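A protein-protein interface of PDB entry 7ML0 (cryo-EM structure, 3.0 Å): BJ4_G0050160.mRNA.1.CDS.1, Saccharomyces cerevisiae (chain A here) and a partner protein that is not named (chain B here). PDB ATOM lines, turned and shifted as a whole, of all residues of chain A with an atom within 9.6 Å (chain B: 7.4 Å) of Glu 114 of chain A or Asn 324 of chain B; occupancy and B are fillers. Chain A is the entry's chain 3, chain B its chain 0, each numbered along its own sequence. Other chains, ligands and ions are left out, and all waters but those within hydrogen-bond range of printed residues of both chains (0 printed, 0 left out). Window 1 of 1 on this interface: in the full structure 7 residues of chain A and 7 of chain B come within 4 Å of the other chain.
NE2 of His 330 of chain B is in hydrogen-bond range of O of Glu 111 of chain A (3.4 Å).
NE2 of His 330 of chain B lies within hydrogen-bond range of N of Asp 115 of chain A (3.1 Å).
OD1 of Asn 324 of chain B lies close to O of Pro 322 of chain B (3.2 Å).
A ring nitrogen (NE2) of His 330 of chain B sits close to the guanidinium group (NE) of Arg 327 of chain B (3.5 Å).
Asn 107 of chain A touches Ile 321 of chain B.
Asn 107 of chain A touches Gly 323 of chain B (CA to CA, 3.5 Å).
Asn 324 of chain B touches Asn 107 of chain A.
Leu 110 of chain A touches Asn 324 of chain B (O to CB, 3.5 Å).
Glu 111 of chain A touches Asn 324 of chain B (CA to CA, 3.5 Å).
CB of Glu 114 of chain A touches CB of Asn 324 of chain B (3.5 Å).
Glu 114 of chain A touches His 330 of chain B.
Arg 327 of chain B touches Asp 115 of chain A.
Tyr 118 of chain A touches Arg 327 of chain B (CB to NH2, 3.2 Å).
Tyr 118 of chain A touches His 330 of chain B.
Glu 114 of chain A touches just these residues of chain B: Asn 324 (3.5 Å) and His 330 (3.1 Å).
Asn 324 of chain B touches just these residues of chain A: Asn 107 (3.7 Å), Leu 110 (3.5 Å), Glu 111 (3.5 Å) and Glu 114 (3.5 Å).
No residue of chain B comes within 4 Å of Val 113 of chain A.
Gly 323 of chain B touches just one residue of chain A: Asn 107.
Printed residues of chain B within 4 Å of Asp 115 of chain A: Arg 327 (3.2 Å) and His 330 (3.1 Å).
Printed residues of chain B within 4 Å of Tyr 118 of chain A: Arg 327 (3.2 Å) and His 330 (3.3 Å).
Of the printed residues of chain B, Asn 107 of chain A touches Ile 321, Gly 323 and Asn 324.
Of the printed residues of chain A, His 330 of chain B touches Glu 111, Glu 114, Asp 115 and Tyr 118.
Printed residues of chain B within 4 Å of Glu 111 of chain A: Asn 324 (3.5 Å) and His 330 (3.4 Å).
Thr 95 of chain A touches none of the printed residues of chain B.
Phe 89 of chain A touches none of the printed residues of chain B.
The nearest residue of chain B that does not touch Glu 114 of chain A is Arg 327 of chain B (4.4 Å).
Of the 30 printed residues of chain A, 6 touch a printed residue of chain B.
Printed residues of chain A that touch a printed residue of chain B: Asn 107, Leu 110, Glu 111, Glu 114, Asp 115 and Tyr 118.
Of the 16 printed residues of chain B, 5 touch a printed residue of chain A.
Printed residues of chain B that touch a printed residue of chain A: Ile 321, Gly 323, Asn 324, Arg 327 and His 330.
Hydrophobic or aromatic side chains of chain B within 4 Å of the printed part of chain A: Ile 321 and His 330.
Among the printed residues, no Asp or Glu carboxylate lies within 4 Å of a Lys or Arg side-chain nitrogen of the other chain.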
ATOM      1  N   GLU A  81      25.593 -18.641  23.670  1.00  0.00           N
ATOM      2  CA  GLU A  81      24.222 -18.157  23.654  1.00  0.00           C
ATOM      3  C   GLU A  81      24.167 -16.718  24.129  1.00  0.00           C
ATOM      4  O   GLU A  81      23.464 -15.887  23.544  1.00  0.00           O
ATOM      5  CB  GLU A  81      23.338 -19.044  24.527  1.00  0.00           C
ATOM      6  N   ILE A  84      25.469 -15.169  21.316  1.00  0.00           N
ATOM      7  CA  ILE A  84      24.354 -15.178  20.377  1.00  0.00           C
ATOM      8  C   ILE A  84      23.341 -14.122  20.778  1.00  0.00           C
ATOM      9  O   ILE A  84      22.911 -13.302  19.960  1.00  0.00           O
ATOM     10  CB  ILE A  84      23.713 -16.574  20.309  1.00  0.00           C
ATOM     11  N   ARG A  85      22.971 -14.109  22.058  1.00  0.00           N
ATOM     12  CA  ARG A  85      22.138 -13.029  22.556  1.00  0.00           C
ATOM     13  C   ARG A  85      22.835 -11.692  22.376  1.00  0.00           C
ATOM     14  O   ARG A  85      22.235 -10.734  21.883  1.00  0.00           O
ATOM     15  CB  ARG A  85      21.793 -13.265  24.025  1.00  0.00           C
ATOM     16  N   VAL A  88      22.538 -11.023  18.994  1.00  0.00           N
ATOM     17  CA  VAL A  88      21.143 -10.652  18.803  1.00  0.00           C
ATOM     18  C   VAL A  88      20.870  -9.307  19.454  1.00  0.00           C
ATOM     19  O   VAL A  88      20.663  -8.301  18.769  1.00  0.00           O
ATOM     20  CB  VAL A  88      20.214 -11.744  19.358  1.00  0.00           C
ATOM     21  N   PHE A  89      20.979  -9.244  20.771  1.00  0.00           N
ATOM     22  CA  PHE A  89      20.613  -8.039  21.508  1.00  0.00           C
ATOM     23  C   PHE A  89      21.441  -6.864  21.132  1.00  0.00           C
ATOM     24  O   PHE A  89      21.281  -5.802  21.735  1.00  0.00           O
ATOM     25  CB  PHE A  89      20.720  -8.285  23.013  1.00  0.00           C
ATOM     26  N   PHE A  92      19.313  -7.530  17.053  1.00  0.00           N
ATOM     27  CA  PHE A  92      17.975  -7.843  17.539  1.00  0.00           C
ATOM     28  C   PHE A  92      17.592  -6.991  18.727  1.00  0.00           C
ATOM     29  O   PHE A  92      16.497  -7.160  19.267  1.00  0.00           O
ATOM     30  CB  PHE A  92      17.868  -9.322  17.910  1.00  0.00           C
ATOM     31  N   THR A  95      14.374  -5.333  18.325  1.00  0.00           N
ATOM     32  CA  THR A  95      13.119  -6.011  18.614  1.00  0.00           C
ATOM     33  C   THR A  95      12.117  -5.047  19.238  1.00  0.00           C
ATOM     34  O   THR A  95      12.483  -4.111  19.955  1.00  0.00           O
ATOM     35  CB  THR A  95      13.347  -7.194  19.556  1.00  0.00           C
ATOM     36  N   ASP A  97       9.076  -4.967  21.682  1.00  0.00           N
ATOM     37  CA  ASP A  97       8.100  -5.343  22.696  1.00  0.00           C
ATOM     38  C   ASP A  97       7.550  -4.108  23.396  1.00  0.00           C
ATOM     39  O   ASP A  97       6.338  -3.877  23.386  1.00  0.00           O
ATOM     40  CB  ASP A  97       8.722  -6.309  23.711  1.00  0.00           C
ATOM     41  N   LEU A 103       0.558  -6.816  24.790  1.00  0.00           N
ATOM     42  CA  LEU A 103       1.086  -7.722  25.806  1.00  0.00           C
ATOM     43  C   LEU A 103       1.304  -9.119  25.252  1.00  0.00           C
ATOM     44  O   LEU A 103       2.325  -9.754  25.535  1.00  0.00           O
ATOM     45  CB  LEU A 103       0.141  -7.769  27.002  1.00  0.00           C
ATOM     46  N   VAL A 104       0.363  -9.611  24.452  1.00  0.00           N
ATOM     47  CA  VAL A 104       0.579 -10.880  23.773  1.00  0.00           C
ATOM     48  C   VAL A 104       1.698 -10.742  22.753  1.00  0.00           C
ATOM     49  O   VAL A 104       2.632 -11.551  22.713  1.00  0.00           O
ATOM     50  CB  VAL A 104      -0.724 -11.364  23.117  1.00  0.00           C
ATOM     51  N   GLU A 105       1.627  -9.702  21.921  1.00  0.00           N
ATOM     52  CA  GLU A 105       2.637  -9.522  20.886  1.00  0.00           C
ATOM     53  C   GLU A 105       3.988  -9.195  21.499  1.00  0.00           C
ATOM     54  O   GLU A 105       5.011  -9.768  21.110  1.00  0.00           O
ATOM     55  CB  GLU A 105       2.210  -8.423  19.917  1.00  0.00           C
ATOM     56  N   TYR A 106       4.011  -8.272  22.460  1.00  0.00           N
ATOM     57  CA  TYR A 106       5.247  -8.016  23.184  1.00  0.00           C
ATOM     58  C   TYR A 106       5.771  -9.301  23.801  1.00  0.00           C
ATOM     59  O   TYR A 106       6.981  -9.542  23.825  1.00  0.00           O
ATOM     60  CB  TYR A 106       5.025  -6.949  24.253  1.00  0.00           C
ATOM     61  N   ASN A 107       4.869 -10.148  24.293  1.00  0.00           N
ATOM     62  CA  ASN A 107       5.270 -11.504  24.638  1.00  0.00           C
ATOM     63  C   ASN A 107       5.682 -12.271  23.393  1.00  0.00           C
ATOM     64  O   ASN A 107       6.731 -12.926  23.373  1.00  0.00           O
ATOM     65  CB  ASN A 107       4.132 -12.221  25.358  1.00  0.00           C
ATOM     66  N   LYS A 108       4.875 -12.189  22.336  1.00  0.00           N
ATOM     67  CA  LYS A 108       5.168 -12.948  21.128  1.00  0.00           C
ATOM     68  C   LYS A 108       6.460 -12.471  20.481  1.00  0.00           C
ATOM     69  O   LYS A 108       7.349 -13.275  20.181  1.00  0.00           O
ATOM     70  CB  LYS A 108       4.005 -12.843  20.145  1.00  0.00           C
ATOM     71  N   TYR A 109       6.587 -11.158  20.270  1.00  0.00           N
ATOM     72  CA  TYR A 109       7.781 -10.635  19.618  1.00  0.00           C
ATOM     73  C   TYR A 109       9.025 -11.000  20.407  1.00  0.00           C
ATOM     74  O   TYR A 109      10.044 -11.394  19.830  1.00  0.00           O
ATOM     75  CB  TYR A 109       7.675  -9.121  19.456  1.00  0.00           C
ATOM     76  N   LEU A 110       8.955 -10.885  21.732  1.00  0.00           N
ATOM     77  CA  LEU A 110      10.024 -11.415  22.567  1.00  0.00           C
ATOM     78  C   LEU A 110      10.187 -12.908  22.333  1.00  0.00           C
ATOM     79  O   LEU A 110      11.294 -13.390  22.070  1.00  0.00           O
ATOM     80  CB  LEU A 110       9.738 -11.127  24.041  1.00  0.00           C
ATOM     81  N   GLU A 111       9.083 -13.655  22.399  1.00  0.00           N
ATOM     82  CA  GLU A 111       9.154 -15.075  22.090  1.00  0.00           C
ATOM     83  C   GLU A 111       9.709 -15.284  20.694  1.00  0.00           C
ATOM     84  O   GLU A 111      10.578 -16.138  20.484  1.00  0.00           O
ATOM     85  CB  GLU A 111       7.775 -15.715  22.227  1.00  0.00           C
ATOM     86  N   GLU A 112       9.252 -14.479  19.736  1.00  0.00           N
ATOM     87  CA  GLU A 112       9.758 -14.582  18.373  1.00  0.00           C
ATOM     88  C   GLU A 112      11.251 -14.304  18.326  1.00  0.00           C
ATOM     89  O   GLU A 112      12.026 -15.088  17.766  1.00  0.00           O
ATOM     90  CB  GLU A 112       9.007 -13.612  17.463  1.00  0.00           C
ATOM     91  N   VAL A 113      11.672 -13.187  18.914  1.00  0.00           N
ATOM     92  CA  VAL A 113      13.093 -12.867  18.939  1.00  0.00           C
ATOM     93  C   VAL A 113      13.855 -13.969  19.655  1.00  0.00           C
ATOM     94  O   VAL A 113      14.889 -14.449  19.178  1.00  0.00           O
ATOM     95  CB  VAL A 113      13.321 -11.499  19.602  1.00  0.00           C
ATOM     96  N   GLU A 114      13.338 -14.399  20.803  1.00  0.00           N
ATOM     97  CA  GLU A 114      13.992 -15.473  21.535  1.00  0.00           C
ATOM     98  C   GLU A 114      13.972 -16.765  20.742  1.00  0.00           C
ATOM     99  O   GLU A 114      14.967 -17.493  20.713  1.00  0.00           O
ATOM    100  CB  GLU A 114      13.326 -15.667  22.890  1.00  0.00           C
ATOM    101  N   ASP A 115      12.849 -17.071  20.094  1.00  0.00           N
ATOM    102  CA  ASP A 115      12.823 -18.232  19.219  1.00  0.00           C
ATOM    103  C   ASP A 115      13.863 -18.094  18.124  1.00  0.00           C
ATOM    104  O   ASP A 115      14.578 -19.052  17.808  1.00  0.00           O
ATOM    105  CB  ASP A 115      11.434 -18.415  18.616  1.00  0.00           C
ATOM    106  N   ILE A 116      13.970 -16.900  17.541  1.00  0.00           N
ATOM    107  CA  ILE A 116      15.056 -16.629  16.609  1.00  0.00           C
ATOM    108  C   ILE A 116      16.395 -16.782  17.314  1.00  0.00           C
ATOM    109  O   ILE A 116      17.334 -17.382  16.776  1.00  0.00           O
ATOM    110  CB  ILE A 116      14.895 -15.227  15.996  1.00  0.00           C
ATOM    111  N   ILE A 117      16.505 -16.244  18.526  1.00  0.00           N
ATOM    112  CA  ILE A 117      17.727 -16.420  19.302  1.00  0.00           C
ATOM    113  C   ILE A 117      17.923 -17.887  19.649  1.00  0.00           C
ATOM    114  O   ILE A 117      18.989 -18.459  19.405  1.00  0.00           O
ATOM    115  CB  ILE A 117      17.691 -15.545  20.565  1.00  0.00           C
ATOM    116  N   TYR A 118      16.885 -18.519  20.204  1.00  0.00           N
ATOM    117  CA  TYR A 118      16.999 -19.919  20.596  1.00  0.00           C
ATOM    118  C   TYR A 118      17.408 -20.776  19.416  1.00  0.00           C
ATOM    119  O   TYR A 118      18.212 -21.701  19.562  1.00  0.00           O
ATOM    120  CB  TYR A 118      15.682 -20.422  21.179  1.00  0.00           C
ATOM    121  N   LYS A 119      16.871 -20.479  18.237  1.00  0.00           N
ATOM    122  CA  LYS A 119      17.308 -21.178  17.039  1.00  0.00           C
ATOM    123  C   LYS A 119      18.816 -21.079  16.885  1.00  0.00           C
ATOM    124  O   LYS A 119      19.512 -22.092  16.758  1.00  0.00           O
ATOM    125  CB  LYS A 119      16.601 -20.596  15.817  1.00  0.00           C
ATOM    126  N   LEU A 120      19.343 -19.858  16.924  1.00  0.00           N
ATOM    127  CA  LEU A 120      20.786 -19.699  16.991  1.00  0.00           C
ATOM    128  C   LEU A 120      21.326 -20.287  18.282  1.00  0.00           C
ATOM    129  O   LEU A 120      22.362 -20.960  18.283  1.00  0.00           O
ATOM    130  CB  LEU A 120      21.155 -18.223  16.877  1.00  0.00           C
ATOM    131  N   ASP A 121      20.616 -20.066  19.389  1.00  0.00           N
ATOM    132  CA  ASP A 121      21.134 -20.460  20.692  1.00  0.00           C
ATOM    133  C   ASP A 121      21.102 -21.972  20.872  1.00  0.00           C
ATOM    134  O   ASP A 121      22.133 -22.585  21.172  1.00  0.00           O
ATOM    135  CB  ASP A 121      20.345 -19.773  21.804  1.00  0.00           C
ATOM    136  N   HIS A 122      19.928 -22.592  20.700  1.00  0.00           N
ATOM    137  CA  HIS A 122      19.832 -24.034  20.908  1.00  0.00           C
ATOM    138  C   HIS A 122      20.860 -24.763  20.063  1.00  0.00           C
ATOM    139  O   HIS A 122      21.400 -25.794  20.479  1.00  0.00           O
ATOM    140  CB  HIS A 122      18.421 -24.531  20.593  1.00  0.00           C
ATOM    141  N   GLY A 123      21.138 -24.243  18.868  1.00  0.00           N
ATOM    142  CA  GLY A 123      22.312 -24.606  18.100  1.00  0.00           C
ATOM    143  C   GLY A 123      22.468 -26.080  17.786  1.00  0.00           C
ATOM    144  O   GLY A 123      23.461 -26.481  17.173  1.00  0.00           O
ATOM    145  N   LYS A 132      17.948 -18.320   9.805  1.00  0.00           N
ATOM    146  CA  LYS A 132      17.751 -17.160  10.655  1.00  0.00           C
ATOM    147  C   LYS A 132      18.962 -16.243  10.621  1.00  0.00           C
ATOM    148  O   LYS A 132      18.823 -15.042  10.843  1.00  0.00           O
ATOM    149  CB  LYS A 132      17.450 -17.591  12.087  1.00  0.00           C
ATOM    150  N   TYR B 286       3.068 -24.937  27.034  1.00  0.00           N
ATOM    151  CA  TYR B 286       3.206 -23.654  26.352  1.00  0.00           C
ATOM    152  C   TYR B 286       1.841 -23.133  25.938  1.00  0.00           C
ATOM    153  O   TYR B 286       1.569 -21.930  26.017  1.00  0.00           O
ATOM    154  CB  TYR B 286       4.104 -23.784  25.121  1.00  0.00           C
ATOM    155  CG  TYR B 286       5.574 -23.996  25.391  1.00  0.00           C
ATOM    156  CD1 TYR B 286       6.066 -24.053  26.685  1.00  0.00           C
ATOM    157  CD2 TYR B 286       6.473 -24.121  24.340  1.00  0.00           C
ATOM    158  CE1 TYR B 286       7.410 -24.241  26.925  1.00  0.00           C
ATOM    159  CE2 TYR B 286       7.818 -24.307  24.569  1.00  0.00           C
ATOM    160  CZ  TYR B 286       8.282 -24.371  25.863  1.00  0.00           C
ATOM    161  OH  TYR B 286       9.627 -24.551  26.097  1.00  0.00           O
ATOM    162  N   ILE B 321       2.267 -12.614  30.688  1.00  0.00           N
ATOM    163  CA  ILE B 321       3.033 -13.854  30.622  1.00  0.00           C
ATOM    164  C   ILE B 321       4.512 -13.498  30.679  1.00  0.00           C
ATOM    165  O   ILE B 321       4.872 -12.330  30.484  1.00  0.00           O
ATOM    166  CB  ILE B 321       2.682 -14.659  29.358  1.00  0.00           C
ATOM    167  CG1 ILE B 321       3.637 -14.332  28.209  1.00  0.00           C
ATOM    168  CG2 ILE B 321       1.245 -14.386  28.931  1.00  0.00           C
ATOM    169  CD1 ILE B 321       3.530 -15.286  27.030  1.00  0.00           C
ATOM    170  N   PRO B 322       5.394 -14.436  30.946  1.00  0.00           N
ATOM    171  CA  PRO B 322       6.830 -14.140  30.920  1.00  0.00           C
ATOM    172  C   PRO B 322       7.365 -14.005  29.498  1.00  0.00           C
ATOM    173  O   PRO B 322       8.453 -14.487  29.176  1.00  0.00           O
ATOM    174  CB  PRO B 322       7.434 -15.346  31.642  1.00  0.00           C
ATOM    175  CG  PRO B 322       6.478 -16.452  31.358  1.00  0.00           C
ATOM    176  CD  PRO B 322       5.129 -15.805  31.423  1.00  0.00           C
ATOM    177  N   GLY B 323       6.604 -13.317  28.653  1.00  0.00           N
ATOM    178  CA  GLY B 323       6.973 -13.074  27.278  1.00  0.00           C
ATOM    179  C   GLY B 323       7.524 -14.292  26.582  1.00  0.00           C
ATOM    180  O   GLY B 323       6.840 -15.296  26.373  1.00  0.00           O
ATOM    181  N   ASN B 324       8.799 -14.187  26.232  1.00  0.00           N
ATOM    182  CA  ASN B 324       9.511 -15.275  25.581  1.00  0.00           C
ATOM    183  C   ASN B 324       9.587 -16.510  26.466  1.00  0.00           C
ATOM    184  O   ASN B 324       9.380 -17.635  25.997  1.00  0.00           O
ATOM    185  CB  ASN B 324      10.904 -14.782  25.240  1.00  0.00           C
ATOM    186  CG  ASN B 324      11.417 -13.818  26.280  1.00  0.00           C
ATOM    187  OD1 ASN B 324      11.058 -13.914  27.454  1.00  0.00           O
ATOM    188  ND2 ASN B 324      12.234 -12.865  25.856  1.00  0.00           N
ATOM    189  N   ILE B 325       9.878 -16.317  27.750  1.00  0.00           N
ATOM    190  CA  ILE B 325      10.132 -17.398  28.696  1.00  0.00           C
ATOM    191  C   ILE B 325       8.959 -18.371  28.725  1.00  0.00           C
ATOM    192  O   ILE B 325       9.092 -19.512  29.185  1.00  0.00           O
ATOM    193  CB  ILE B 325      10.448 -16.806  30.085  1.00  0.00           C
ATOM    194  CG1 ILE B 325      11.949 -16.525  30.193  1.00  0.00           C
ATOM    195  CG2 ILE B 325       9.963 -17.685  31.232  1.00  0.00           C
ATOM    196  CD1 ILE B 325      12.375 -15.960  31.533  1.00  0.00           C
ATOM    197  N   ARG B 326       7.814 -17.939  28.191  1.00  0.00           N
ATOM    198  CA  ARG B 326       6.733 -18.863  27.877  1.00  0.00           C
ATOM    199  C   ARG B 326       7.285 -20.140  27.265  1.00  0.00           C
ATOM    200  O   ARG B 326       6.835 -21.243  27.583  1.00  0.00           O
ATOM    201  CB  ARG B 326       5.739 -18.205  26.922  1.00  0.00           C
ATOM    202  CG  ARG B 326       4.543 -19.076  26.589  1.00  0.00           C
ATOM    203  CD  ARG B 326       3.975 -18.743  25.220  1.00  0.00           C
ATOM    204  NE  ARG B 326       4.815 -19.261  24.139  1.00  0.00           N
ATOM    205  CZ  ARG B 326       4.532 -20.348  23.428  1.00  0.00           C
ATOM    206  NH1 ARG B 326       3.421 -21.032  23.672  1.00  0.00           N
ATOM    207  NH2 ARG B 326       5.354 -20.746  22.468  1.00  0.00           N
ATOM    208  N   ARG B 327       8.286 -20.009  26.404  1.00  0.00           N
ATOM    209  CA  ARG B 327       9.081 -21.164  26.021  1.00  0.00           C
ATOM    210  C   ARG B 327      10.040 -21.505  27.153  1.00  0.00           C
ATOM    211  O   ARG B 327      10.856 -20.671  27.559  1.00  0.00           O
ATOM    212  CB  ARG B 327       9.845 -20.892  24.729  1.00  0.00           C
ATOM    213  CG  ARG B 327      11.044 -21.806  24.518  1.00  0.00           C
ATOM    214  CD  ARG B 327      10.938 -22.615  23.236  1.00  0.00           C
ATOM    215  NE  ARG B 327      11.302 -21.856  22.038  1.00  0.00           N
ATOM    216  CZ  ARG B 327      12.467 -21.968  21.404  1.00  0.00           C
ATOM    217  NH1 ARG B 327      13.396 -22.800  21.852  1.00  0.00           N
ATOM    218  NH2 ARG B 327      12.706 -21.243  20.322  1.00  0.00           N
ATOM    219  N   ALA B 328       9.929 -22.727  27.669  1.00  0.00           N
ATOM    220  CA  ALA B 328      10.792 -23.150  28.761  1.00  0.00           C
ATOM    221  C   ALA B 328      12.249 -23.122  28.335  1.00  0.00           C
ATOM    222  O   ALA B 328      13.136 -22.816  29.138  1.00  0.00           O
ATOM    223  CB  ALA B 328      10.391 -24.543  29.237  1.00  0.00           C
ATOM    224  N   GLU B 329      12.513 -23.440  27.072  1.00  0.00           N
ATOM    225  CA  GLU B 329      13.877 -23.361  26.573  1.00  0.00           C
ATOM    226  C   GLU B 329      14.390 -21.931  26.640  1.00  0.00           C
ATOM    227  O   GLU B 329      15.533 -21.691  27.042  1.00  0.00           O
ATOM    228  CB  GLU B 329      13.934 -23.915  25.153  1.00  0.00           C
ATOM    229  CG  GLU B 329      13.054 -25.157  24.970  1.00  0.00           C
ATOM    230  CD  GLU B 329      13.232 -26.187  26.081  1.00  0.00           C
ATOM    231  OE1 GLU B 329      14.388 -26.535  26.400  1.00  0.00           O
ATOM    232  OE2 GLU B 329      12.215 -26.640  26.646  1.00  0.00           O
ATOM    233  N   HIS B 330      13.547 -20.962  26.274  1.00  0.00           N
ATOM    234  CA  HIS B 330      13.820 -19.583  26.654  1.00  0.00           C
ATOM    235  C   HIS B 330      13.966 -19.479  28.163  1.00  0.00           C
ATOM    236  O   HIS B 330      14.933 -18.903  28.673  1.00  0.00           O
ATOM    237  CB  HIS B 330      12.698 -18.660  26.167  1.00  0.00           C
ATOM    238  CG  HIS B 330      12.491 -18.669  24.682  1.00  0.00           C
ATOM    239  ND1 HIS B 330      13.391 -19.233  23.806  1.00  0.00           N
ATOM    240  CD2 HIS B 330      11.484 -18.178  23.920  1.00  0.00           C
ATOM    241  CE1 HIS B 330      12.948 -19.089  22.570  1.00  0.00           C
ATOM    242  NE2 HIS B 330      11.792 -18.455  22.612  1.00  0.00           N
ATOM    243  N   PHE B 331      13.022 -20.073  28.893  1.00  0.00           N
ATOM    244  CA  PHE B 331      13.003 -19.960  30.346  1.00  0.00           C
ATOM    245  C   PHE B 331      14.232 -20.598  30.974  1.00  0.00           C
ATOM    246  O   PHE B 331      14.898 -19.990  31.820  1.00  0.00           O
ATOM    247  CB  PHE B 331      11.732 -20.605  30.875  1.00  0.00           C
ATOM    248  CG  PHE B 331      11.785 -20.957  32.317  1.00  0.00           C
ATOM    249  CD1 PHE B 331      11.767 -19.972  33.282  1.00  0.00           C
ATOM    250  CD2 PHE B 331      11.817 -22.278  32.715  1.00  0.00           C
ATOM    251  CE1 PHE B 331      11.788 -20.297  34.619  1.00  0.00           C
ATOM    252  CE2 PHE B 331      11.838 -22.607  34.050  1.00  0.00           C
ATOM    253  CZ  PHE B 331      11.821 -21.616  35.004  1.00  0.00           C
ATOM    254  N   SER B 333      17.127 -21.102  29.755  1.00  0.00           N
ATOM    255  CA  SER B 333      18.345 -20.370  29.441  1.00  0.00           C
ATOM    256  C   SER B 333      18.591 -19.241  30.430  1.00  0.00           C
ATOM    257  O   SER B 333      19.674 -19.139  31.016  1.00  0.00           O
ATOM    258  CB  SER B 333      18.250 -19.820  28.027  1.00  0.00           C
ATOM    259  OG  SER B 333      17.106 -18.996  27.918  1.00  0.00           O
ATOM    260  N   PHE B 334      17.591 -18.383  30.636  1.00  0.00           N
ATOM    261  CA  PHE B 334      17.797 -17.234  31.510  1.00  0.00           C
ATOM    262  C   PHE B 334      18.090 -17.659  32.934  1.00  0.00           C
ATOM    263  O   PHE B 334      18.758 -16.932  33.675  1.00  0.00           O
ATOM    264  CB  PHE B 334      16.583 -16.316  31.478  1.00  0.00           C
ATOM    265  CG  PHE B 334      16.719 -15.173  30.523  1.00  0.00           C
ATOM    266  CD1 PHE B 334      17.501 -14.079  30.840  1.00  0.00           C
ATOM    267  CD2 PHE B 334      16.063 -15.183  29.312  1.00  0.00           C
ATOM    268  CE1 PHE B 334      17.629 -13.024  29.962  1.00  0.00           C
ATOM    269  CE2 PHE B 334      16.193 -14.131  28.432  1.00  0.00           C
ATOM    270  CZ  PHE B 334      16.975 -13.049  28.762  1.00  0.00           C
ATOM    271  N   PRO B 373      10.113 -10.852  34.059  1.00  0.00           N
ATOM    272  CA  PRO B 373      10.226 -12.314  34.102  1.00  0.00           C
ATOM    273  C   PRO B 373      10.669 -12.820  35.447  1.00  0.00           C
ATOM    274  O   PRO B 373      10.316 -13.942  35.834  1.00  0.00           O
ATOM    275  CB  PRO B 373      11.278 -12.617  33.030  1.00  0.00           C
ATOM    276  CG  PRO B 373      11.371 -11.393  32.212  1.00  0.00           C
ATOM    277  CD  PRO B 373      11.070 -10.266  33.113  1.00  0.00           C
ATOM    278  N   ARG B 380       6.780 -20.453  36.930  1.00  0.00           N
ATOM    279  CA  ARG B 380       7.309 -21.055  35.718  1.00  0.00           C
ATOM    280  C   ARG B 380       8.165 -22.258  36.064  1.00  0.00           C
ATOM    281  O   ARG B 380       8.079 -23.306  35.415  1.00  0.00           O
ATOM    282  CB  ARG B 380       8.113 -20.019  34.941  1.00  0.00           C
ATOM    283  CG  ARG B 380       8.416 -20.396  33.514  1.00  0.00           C
ATOM    284  CD  ARG B 380       7.203 -20.237  32.624  1.00  0.00           C
ATOM    285  NE  ARG B 380       7.530 -20.504  31.228  1.00  0.00           N
ATOM    286  CZ  ARG B 380       7.681 -21.724  30.728  1.00  0.00           C
ATOM    287  NH1 ARG B 380       7.539 -22.788  31.502  1.00  0.00           N
ATOM    288  NH2 ARG B 380       7.973 -21.884  29.452  1.00  0.00           N
